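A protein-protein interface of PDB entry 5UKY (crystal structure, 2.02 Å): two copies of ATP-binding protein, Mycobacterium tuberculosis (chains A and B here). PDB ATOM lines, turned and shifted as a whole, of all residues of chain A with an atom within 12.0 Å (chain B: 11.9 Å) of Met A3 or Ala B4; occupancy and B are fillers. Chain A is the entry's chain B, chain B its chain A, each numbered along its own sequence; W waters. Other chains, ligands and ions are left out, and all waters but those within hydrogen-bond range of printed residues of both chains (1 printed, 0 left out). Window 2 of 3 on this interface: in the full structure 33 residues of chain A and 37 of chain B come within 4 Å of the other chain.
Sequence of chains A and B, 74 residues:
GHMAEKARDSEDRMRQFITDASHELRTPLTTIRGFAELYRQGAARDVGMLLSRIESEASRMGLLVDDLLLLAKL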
ATOM      1  N   GLY A   1      24.121  -5.078  12.350  1.00  0.00           N
ATOM      2  CA  GLY A   1      25.598  -4.888  12.402  1.00  0.00           C
ATOM      3  C   GLY A   1      26.190  -4.698  11.023  1.00  0.00           C
ATOM      4  O   GLY A   1      25.534  -4.130  10.147  1.00  0.00           O
ATOM      5  N   HIS A   2      27.427  -5.176  10.829  1.00  0.00           N
ATOM      6  CA  HIS A   2      28.188  -4.972   9.575  1.00  0.00           C
ATOM      7  C   HIS A   2      27.588  -5.689   8.368  1.00  0.00           C
ATOM      8  O   HIS A   2      27.701  -5.194   7.239  1.00  0.00           O
ATOM      9  CB  HIS A   2      29.649  -5.425   9.723  1.00  0.00           C
ATOM     10  CG  HIS A   2      30.527  -5.051   8.561  1.00  0.00           C
ATOM     11  ND1 HIS A   2      31.143  -3.817   8.453  1.00  0.00           N
ATOM     12  CD2 HIS A   2      30.902  -5.756   7.467  1.00  0.00           C
ATOM     13  CE1 HIS A   2      31.856  -3.780   7.341  1.00  0.00           C
ATOM     14  NE2 HIS A   2      31.724  -4.942   6.723  1.00  0.00           N
ATOM     15  N   MET A   3      26.957  -6.840   8.597  1.00  0.00           N
ATOM     16  CA  MET A   3      26.374  -7.621   7.489  1.00  0.00           C
ATOM     17  C   MET A   3      25.109  -6.910   6.911  1.00  0.00           C
ATOM     18  O   MET A   3      24.986  -6.735   5.691  1.00  0.00           O
ATOM     19  CB  MET A   3      26.111  -9.078   7.932  1.00  0.00           C
ATOM     20  CG  MET A   3      27.330  -9.807   8.524  1.00  0.00           C
ATOM     21  SD  MET A   3      28.694 -10.112   7.361  1.00  0.00           S
ATOM     22  CE  MET A   3      30.127 -10.093   8.448  1.00  0.00           C
ATOM     23  N   ALA A   4      24.214  -6.458   7.792  1.00  0.00           N
ATOM     24  CA  ALA A   4      23.060  -5.600   7.408  1.00  0.00           C
ATOM     25  C   ALA A   4      23.498  -4.284   6.744  1.00  0.00           C
ATOM     26  O   ALA A   4      22.970  -3.913   5.701  1.00  0.00           O
ATOM     27  CB  ALA A   4      22.161  -5.300   8.615  1.00  0.00           C
ATOM     28  N   GLU A   5      24.470  -3.610   7.357  1.00  0.00           N
ATOM     29  CA  GLU A   5      25.062  -2.387   6.814  1.00  0.00           C
ATOM     30  C   GLU A   5      25.474  -2.544   5.338  1.00  0.00           C
ATOM     31  O   GLU A   5      25.195  -1.658   4.537  1.00  0.00           O
ATOM     32  CB  GLU A   5      26.274  -1.950   7.667  1.00  0.00           C
ATOM     33  CG  GLU A   5      26.765  -0.524   7.425  1.00  0.00           C
ATOM     34  CD  GLU A   5      28.031  -0.437   6.584  1.00  0.00           C
ATOM     35  OE1 GLU A   5      29.112  -0.876   7.056  1.00  0.00           O
ATOM     36  OE2 GLU A   5      27.945   0.097   5.458  1.00  0.00           O
ATOM     37  N   LYS A   6      26.113  -3.662   4.984  1.00  0.00           N
ATOM     38  CA  LYS A   6      26.569  -3.875   3.604  1.00  0.00           C
ATOM     39  C   LYS A   6      25.447  -4.304   2.652  1.00  0.00           C
ATOM     40  O   LYS A   6      25.402  -3.836   1.517  1.00  0.00           O
ATOM     41  CB  LYS A   6      27.768  -4.837   3.544  1.00  0.00           C
ATOM     42  CG  LYS A   6      29.090  -4.258   4.102  1.00  0.00           C
ATOM     43  CD  LYS A   6      29.290  -2.755   3.827  1.00  0.00           C
ATOM     44  CE  LYS A   6      30.714  -2.269   4.046  1.00  0.00           C
ATOM     45  NZ  LYS A   6      31.629  -2.672   2.943  1.00  0.00           N
ATOM     46  N   ALA A   7      24.536  -5.157   3.116  1.00  0.00           N
ATOM     47  CA  ALA A   7      23.303  -5.424   2.374  1.00  0.00           C
ATOM     48  C   ALA A   7      22.576  -4.104   2.054  1.00  0.00           C
ATOM     49  O   ALA A   7      22.195  -3.855   0.891  1.00  0.00           O
ATOM     50  CB  ALA A   7      22.401  -6.383   3.143  1.00  0.00           C
ATOM     51  N   ARG A   8      22.442  -3.251   3.071  1.00  0.00           N
ATOM     52  CA  ARG A   8      21.805  -1.943   2.910  1.00  0.00           C
ATOM     53  C   ARG A   8      22.572  -0.951   2.006  1.00  0.00           C
ATOM     54  O   ARG A   8      21.957  -0.286   1.155  1.00  0.00           O
ATOM     55  CB  ARG A   8      21.538  -1.322   4.288  1.00  0.00           C
ATOM     56  CG  ARG A   8      20.906   0.070   4.297  1.00  0.00           C
ATOM     57  CD  ARG A   8      19.716   0.223   3.348  1.00  0.00           C
ATOM     58  NE  ARG A   8      18.651   1.022   3.940  1.00  0.00           N
ATOM     59  CZ  ARG A   8      18.693   2.336   4.157  1.00  0.00           C
ATOM     60  NH1 ARG A   8      19.760   3.059   3.824  1.00  0.00           N
ATOM     61  NH2 ARG A   8      17.648   2.939   4.723  1.00  0.00           N
ATOM     62  N   ASP A   9      23.888  -0.835   2.194  1.00  0.00           N
ATOM     63  CA  ASP A   9      24.712  -0.033   1.298  1.00  0.00           C
ATOM     64  C   ASP A   9      24.614  -0.556  -0.126  1.00  0.00           C
ATOM     65  O   ASP A   9      24.576   0.238  -1.079  1.00  0.00           O
ATOM     66  CB  ASP A   9      26.185   0.030   1.743  1.00  0.00           C
ATOM     67  CG  ASP A   9      27.118   0.589   0.651  1.00  0.00           C
ATOM     68  OD1 ASP A   9      27.156   1.838   0.452  1.00  0.00           O
ATOM     69  OD2 ASP A   9      27.776  -0.230  -0.040  1.00  0.00           O
ATOM     70  N   SER A  10      24.608  -1.880  -0.284  1.00  0.00           N
ATOM     71  CA  SER A  10      24.490  -2.476  -1.608  1.00  0.00           C
ATOM     72  C   SER A  10      23.138  -2.098  -2.244  1.00  0.00           C
ATOM     73  O   SER A  10      23.080  -1.579  -3.367  1.00  0.00           O
ATOM     74  CB  SER A  10      24.666  -3.979  -1.533  1.00  0.00           C
ATOM     75  OG  SER A  10      24.305  -4.586  -2.754  1.00  0.00           O
ATOM     76  N   GLU A  11      22.068  -2.308  -1.492  1.00  0.00           N
ATOM     77  CA  GLU A  11      20.704  -1.898  -1.888  1.00  0.00           C
ATOM     78  C   GLU A  11      20.559  -0.431  -2.282  1.00  0.00           C
ATOM     79  O   GLU A  11      19.927  -0.135  -3.292  1.00  0.00           O
ATOM     80  CB  GLU A  11      19.702  -2.260  -0.806  1.00  0.00           C
ATOM     81  CG  GLU A  11      18.270  -1.843  -1.113  1.00  0.00           C
ATOM     82  CD  GLU A  11      17.362  -1.896   0.098  1.00  0.00           C
ATOM     83  OE1 GLU A  11      16.582  -0.942   0.285  1.00  0.00           O
ATOM     84  OE2 GLU A  11      17.433  -2.888   0.866  1.00  0.00           O
ATOM     85  N   ASP A  12      21.124   0.461  -1.475  1.00  0.00           N
ATOM     86  CA  ASP A  12      21.124   1.908  -1.725  1.00  0.00           C
ATOM     87  C   ASP A  12      21.895   2.347  -2.967  1.00  0.00           C
ATOM     88  O   ASP A  12      21.473   3.267  -3.657  1.00  0.00           O
ATOM     89  CB  ASP A  12      21.722   2.629  -0.545  1.00  0.00           C
ATOM     90  CG  ASP A  12      20.741   2.849   0.576  1.00  0.00           C
ATOM     91  OD1 ASP A  12      19.558   2.397   0.545  1.00  0.00           O
ATOM     92  OD2 ASP A  12      21.192   3.516   1.520  1.00  0.00           O
ATOM     93  N   MET A  14      22.263   0.275  -5.559  1.00  0.00           N
ATOM     94  CA  MET A  14      21.387  -0.230  -6.627  1.00  0.00           C
ATOM     95  C   MET A  14      20.241   0.739  -6.896  1.00  0.00           C
ATOM     96  O   MET A  14      19.924   1.016  -8.041  1.00  0.00           O
ATOM     97  CB  MET A  14      20.841  -1.621  -6.294  1.00  0.00           C
ATOM     98  CG  MET A  14      21.726  -2.734  -6.824  1.00  0.00           C
ATOM     99  SD  MET A  14      21.132  -4.367  -6.377  1.00  0.00           S
ATOM    100  CE  MET A  14      21.577  -4.397  -4.653  1.00  0.00           C
ATOM    101  N   GLY B   1      22.463 -11.851  13.052  1.00  0.00           N
ATOM    102  CA  GLY B   1      21.487 -12.740  12.351  1.00  0.00           C
ATOM    103  C   GLY B   1      20.306 -12.004  11.735  1.00  0.00           C
ATOM    104  O   GLY B   1      20.296 -11.771  10.537  1.00  0.00           O
ATOM    105  N   HIS B   2      19.314 -11.666  12.557  1.00  0.00           N
ATOM    106  CA  HIS B   2      18.006 -11.144  12.108  1.00  0.00           C
ATOM    107  C   HIS B   2      18.090  -9.895  11.251  1.00  0.00           C
ATOM    108  O   HIS B   2      17.413  -9.831  10.225  1.00  0.00           O
ATOM    109  CB  HIS B   2      17.059 -10.871  13.296  1.00  0.00           C
ATOM    110  CG  HIS B   2      16.519 -12.118  13.933  1.00  0.00           C
ATOM    111  ND1 HIS B   2      16.869 -13.375  13.491  1.00  0.00           N
ATOM    112  CD2 HIS B   2      15.703 -12.307  15.008  1.00  0.00           C
ATOM    113  CE1 HIS B   2      16.274 -14.284  14.243  1.00  0.00           C
ATOM    114  NE2 HIS B   2      15.565 -13.667  15.175  1.00  0.00           N
ATOM    115  N   MET B   3      18.912  -8.924  11.655  1.00  0.00           N
ATOM    116  CA  MET B   3      19.042  -7.684  10.871  1.00  0.00           C
ATOM    117  C   MET B   3      19.733  -7.952   9.539  1.00  0.00           C
ATOM    118  O   MET B   3      19.345  -7.387   8.518  1.00  0.00           O
ATOM    119  CB  MET B   3      19.735  -6.550  11.648  1.00  0.00           C
ATOM    120  CG  MET B   3      18.917  -5.260  11.680  1.00  0.00           C
ATOM    121  SD  MET B   3      17.440  -5.431  12.721  1.00  0.00           S
ATOM    122  CE  MET B   3      16.145  -6.007  11.609  1.00  0.00           C
ATOM    123  N   ALA B   4      20.712  -8.847   9.544  1.00  0.00           N
ATOM    124  CA  ALA B   4      21.452  -9.182   8.333  1.00  0.00           C
ATOM    125  C   ALA B   4      20.562  -9.951   7.342  1.00  0.00           C
ATOM    126  O   ALA B   4      20.625  -9.713   6.144  1.00  0.00           O
ATOM    127  CB  ALA B   4      22.696  -9.975   8.660  1.00  0.00           C
ATOM    128  N   GLU B   5      19.713 -10.838   7.851  1.00  0.00           N
ATOM    129  CA  GLU B   5      18.892 -11.690   7.007  1.00  0.00           C
ATOM    130  C   GLU B   5      17.759 -10.865   6.357  1.00  0.00           C
ATOM    131  O   GLU B   5      17.495 -11.021   5.168  1.00  0.00           O
ATOM    132  CB  GLU B   5      18.374 -12.883   7.826  1.00  0.00           C
ATOM    133  CG  GLU B   5      17.571 -13.902   7.039  1.00  0.00           C
ATOM    134  CD  GLU B   5      16.077 -13.751   7.234  1.00  0.00           C
ATOM    135  OE1 GLU B   5      15.310 -14.561   6.642  1.00  0.00           O
ATOM    136  OE2 GLU B   5      15.671 -12.825   7.984  1.00  0.00           O
ATOM    137  N   LYS B   6      17.134  -9.979   7.126  1.00  0.00           N
ATOM    138  CA  LYS B   6      16.160  -9.014   6.619  1.00  0.00           C
ATOM    139  C   LYS B   6      16.740  -7.989   5.639  1.00  0.00           C
ATOM    140  O   LYS B   6      16.075  -7.612   4.658  1.00  0.00           O
ATOM    141  CB  LYS B   6      15.519  -8.241   7.782  1.00  0.00           C
ATOM    142  CG  LYS B   6      14.487  -7.216   7.318  1.00  0.00           C
ATOM    143  CD  LYS B   6      13.260  -7.143   8.205  1.00  0.00           C
ATOM    144  CE  LYS B   6      12.060  -6.583   7.443  1.00  0.00           C
ATOM    145  NZ  LYS B   6      10.804  -6.775   8.218  1.00  0.00           N
ATOM    146  N   ALA B   7      17.943  -7.502   5.937  1.00  0.00           N
ATOM    147  CA  ALA B   7      18.651  -6.640   5.023  1.00  0.00           C
ATOM    148  C   ALA B   7      19.005  -7.387   3.726  1.00  0.00           C
ATOM    149  O   ALA B   7      18.957  -6.782   2.659  1.00  0.00           O
ATOM    150  CB  ALA B   7      19.918  -6.090   5.674  1.00  0.00           C
ATOM    151  N   ARG B   8      19.403  -8.659   3.828  1.00  0.00           N
ATOM    152  CA  ARG B   8      19.733  -9.486   2.654  1.00  0.00           C
ATOM    153  C   ARG B   8      18.485  -9.792   1.807  1.00  0.00           C
ATOM    154  O   ARG B   8      18.564  -9.820   0.585  1.00  0.00           O
ATOM    155  CB  ARG B   8      20.434 -10.824   3.031  1.00  0.00           C
ATOM    156  CG  ARG B   8      21.945 -10.760   3.247  1.00  0.00           C
ATOM    157  CD  ARG B   8      22.672 -12.116   3.119  1.00  0.00           C
ATOM    158  NE  ARG B   8      21.888 -13.304   3.536  1.00  0.00           N
ATOM    159  CZ  ARG B   8      21.754 -13.774   4.788  1.00  0.00           C
ATOM    160  NH1 ARG B   8      22.350 -13.182   5.829  1.00  0.00           N
ATOM    161  NH2 ARG B   8      20.994 -14.852   5.009  1.00  0.00           N
ATOM    162  N   ASP B   9      17.368 -10.082   2.482  1.00  0.00           N
ATOM    163  CA  ASP B   9      16.077 -10.250   1.828  1.00  0.00           C
ATOM    164  C   ASP B   9      15.681  -8.958   1.119  1.00  0.00           C
ATOM    165  O   ASP B   9      15.252  -8.982  -0.020  1.00  0.00           O
ATOM    166  CB  ASP B   9      14.951 -10.606   2.790  1.00  0.00           C
ATOM    167  CG  ASP B   9      13.657 -10.939   2.041  1.00  0.00           C
ATOM    168  OD1 ASP B   9      13.683 -11.877   1.213  1.00  0.00           O
ATOM    169  OD2 ASP B   9      12.632 -10.247   2.223  1.00  0.00           O
ATOM    170  N   SER B  10      15.838  -7.841   1.800  1.00  0.00           N
ATOM    171  CA  SER B  10      15.531  -6.587   1.182  1.00  0.00           C
ATOM    172  C   SER B  10      16.473  -6.334  -0.005  1.00  0.00           C
ATOM    173  O   SER B  10      16.007  -5.990  -1.110  1.00  0.00           O
ATOM    174  CB  SER B  10      15.507  -5.472   2.221  1.00  0.00           C
ATOM    175  OG  SER B  10      15.155  -4.262   1.595  1.00  0.00           O
ATOM    176  N   GLU B  11      17.770  -6.592   0.153  1.00  0.00           N
ATOM    177  CA  GLU B  11      18.687  -6.413  -0.972  1.00  0.00           C
ATOM    178  C   GLU B  11      18.389  -7.354  -2.171  1.00  0.00           C
ATOM    179  O   GLU B  11      18.466  -6.902  -3.316  1.00  0.00           O
ATOM    180  CB  GLU B  11      20.134  -6.541  -0.523  1.00  0.00           C
ATOM    181  CG  GLU B  11      21.156  -6.385  -1.656  1.00  0.00           C
ATOM    182  CD  GLU B  11      22.482  -7.062  -1.395  1.00  0.00           C
ATOM    183  OE1 GLU B  11      23.355  -6.946  -2.281  1.00  0.00           O
ATOM    184  OE2 GLU B  11      22.673  -7.679  -0.321  1.00  0.00           O
ATOM    185  N   ASP B  12      18.032  -8.616  -1.908  1.00  0.00           N
ATOM    186  CA  ASP B  12      17.653  -9.596  -2.952  1.00  0.00           C
ATOM    187  C   ASP B  12      16.389  -9.245  -3.720  1.00  0.00           C
ATOM    188  O   ASP B  12      16.313  -9.465  -4.897  1.00  0.00           O
ATOM    189  CB  ASP B  12      17.432 -11.001  -2.347  1.00  0.00           C
ATOM    190  CG  ASP B  12      18.728 -11.668  -1.896  1.00  0.00           C
ATOM    191  OD1 ASP B  12      19.815 -11.270  -2.341  1.00  0.00           O
ATOM    192  OD2 ASP B  12      18.654 -12.590  -1.071  1.00  0.00           O
ATOM    193  N   ARG B  13      15.406  -8.702  -3.028  1.00  0.00           N
ATOM    194  CA  ARG B  13      14.222  -8.216  -3.662  1.00  0.00           C
ATOM    195  C   ARG B  13      14.594  -7.054  -4.561  1.00  0.00           C
ATOM    196  O   ARG B  13      14.105  -6.989  -5.670  1.00  0.00           O
ATOM    197  CB  ARG B  13      13.156  -7.790  -2.632  1.00  0.00           C
ATOM    198  CG  ARG B  13      12.464  -8.943  -1.920  1.00  0.00           C
ATOM    199  CD  ARG B  13      11.232  -8.425  -1.166  1.00  0.00           C
ATOM    200  NE  ARG B  13      10.211  -8.009  -2.115  1.00  0.00           N
ATOM    201  CZ  ARG B  13       9.422  -8.848  -2.799  1.00  0.00           C
ATOM    202  NH1 ARG B  13       9.483 -10.167  -2.592  1.00  0.00           N
ATOM    203  NH2 ARG B  13       8.533  -8.372  -3.676  1.00  0.00           N
ATOM    204  N   ARG B  15      17.610  -6.585  -6.095  1.00  0.00           N
ATOM    205  CA  ARG B  15      18.211  -7.223  -7.284  1.00  0.00           C
ATOM    206  C   ARG B  15      17.190  -7.771  -8.244  1.00  0.00           C
ATOM    207  O   ARG B  15      17.303  -7.537  -9.438  1.00  0.00           O
ATOM    208  CB  ARG B  15      19.107  -8.405  -6.900  1.00  0.00           C
ATOM    209  CG  ARG B  15      20.407  -7.962  -6.289  1.00  0.00           C
ATOM    210  CD  ARG B  15      21.147  -9.132  -5.676  1.00  0.00           C
ATOM    211  NE  ARG B  15      22.295  -8.613  -4.955  1.00  0.00           N
ATOM    212  CZ  ARG B  15      23.433  -8.252  -5.516  1.00  0.00           C
ATOM    213  NH1 ARG B  15      23.605  -8.365  -6.834  1.00  0.00           N
ATOM    214  NH2 ARG B  15      24.413  -7.780  -4.743  1.00  0.00           N
HETATM  215  O   HOH W   1      19.032  -3.855   2.744  1.00  0.00           O
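The side-chain carboxylate of Glu A11 sits at hydrogen-bond distance from the side-chain hydroxyl of Ser B10 (2.8 Å). The side-chain carboxylate of Glu B11 sits at hydrogen-bond distance from the side-chain hydroxyl of Ser A10 (2.6 Å).
The side-chain carboxylate of Glu B11 is in salt-bridge range of the guanidinium group of Arg B15 (2.8 Å).
Met B3 touches Ala A4. N of Ala A4 touches CA of Ala B4, at 3.9 Å. CB of Ala B7 touches CA of Ala A4, at 3.6 Å. O of Ala B7 touches CB of Ala A7 (3.5 Å). Ala A7 touches Arg B8 (CB to N, 3.8 Å). CA of Ala A7 touches OE2 of Glu B11 (3.6 Å). Ser A10 touches Arg B15. OE2 of Glu A11 touches N of Glu B11, 3.8 Å away. CG of Glu B11 touches CE of Met A14, at 3.6 Å. Met A14 touches Arg B15 (SD to CG, 3.7 Å).
Of chain B, only Ala B4 comes within 4 Å of Met A3. Ala B4 touches just these residues of chain A: Met A3 (3.6 Å) and Ala A4 (3.9 Å). No residue of chain B comes within 4 Å of Gly A1. No residue of chain B comes within 4 Å of His A2. Of chain B, only Met B3 (3.5 Å), Ala B4 (3.9 Å) and Ala B7 (3.6 Å) come within 4 Å of Ala A4. No residue of chain B comes within 4 Å of Glu A5. Of the printed residues of chain A, Met B3 touches Ala A4 (3.5 Å). Ala B7 touches just these residues of chain A: Ala A4 and Ala A7. Of chain A, only Ala A7 (3.8 Å) comes within 4 Å of Arg B8. Of the printed residues of chain A, Ser B10 touches Glu A11 (2.8 Å). Printed residues of chain B within 4 Å of Ser A10: Glu B11 and Arg B15. Of the printed residues of chain B, Glu A11 touches Ser B10 and Glu B11. Printed residues of chain A within 4 Å of Arg B15: Ser A10 and Met A14. Of the printed residues of chain B, Met A14 touches Glu B11 and Arg B15. Asp A12 touches none of the printed residues of chain B. Lys B6 touches none of the printed residues of chain A. The nearest residue of chain B that does not touch Met A3 is Ala B7 (5.1 Å). The nearest residue of chain A that does not touch Ala B4 is Ala A7 (4.8 Å).
Of the 13 printed residues of chain A, 6 touch a printed residue of chain B. Hydrophobic or aromatic side chains of chain A within 4 Å of the printed part of chain B: Met A3, Ala A4, Ala A7 and Met A14. Along chain A the printed residues that touch a printed residue of chain B span positions 3 to 14. Hydrophobic or aromatic side chains of chain B that line the printed part of chain A: Ala B4 and Ala B7. Among the printed residues, 13 pairs touch across the chains. Among the printed residues, no Asp or Glu carboxylate lies within 4 Å of a Lys or Arg side-chain nitrogen of the other chain.
Ala A4 touches Ala B7, but with the chains exchanged Ala A7 does not touch Ala B4 (4.8 Å). Ala A7 touches its own counterpart, Ala B7. Ala A7 touches Glu B11, but with the chains exchanged Glu A11 does not touch Ala B7 (4.5 Å). Ser A10 touches Glu B11, and with the chains exchanged Glu A11 touches Ser B10. Of the 13 pairs that touch across the chains among the printed residues, 7 have their exchanged pair printed and touching as well.
Water W1 lies within hydrogen-bond range of the side-chain carboxylate of Glu A11 (2.6 Å), the backbone carbonyl oxygen of Ala B7 (2.9 Å) and the backbone NH of Arg A8 (3.5 Å).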
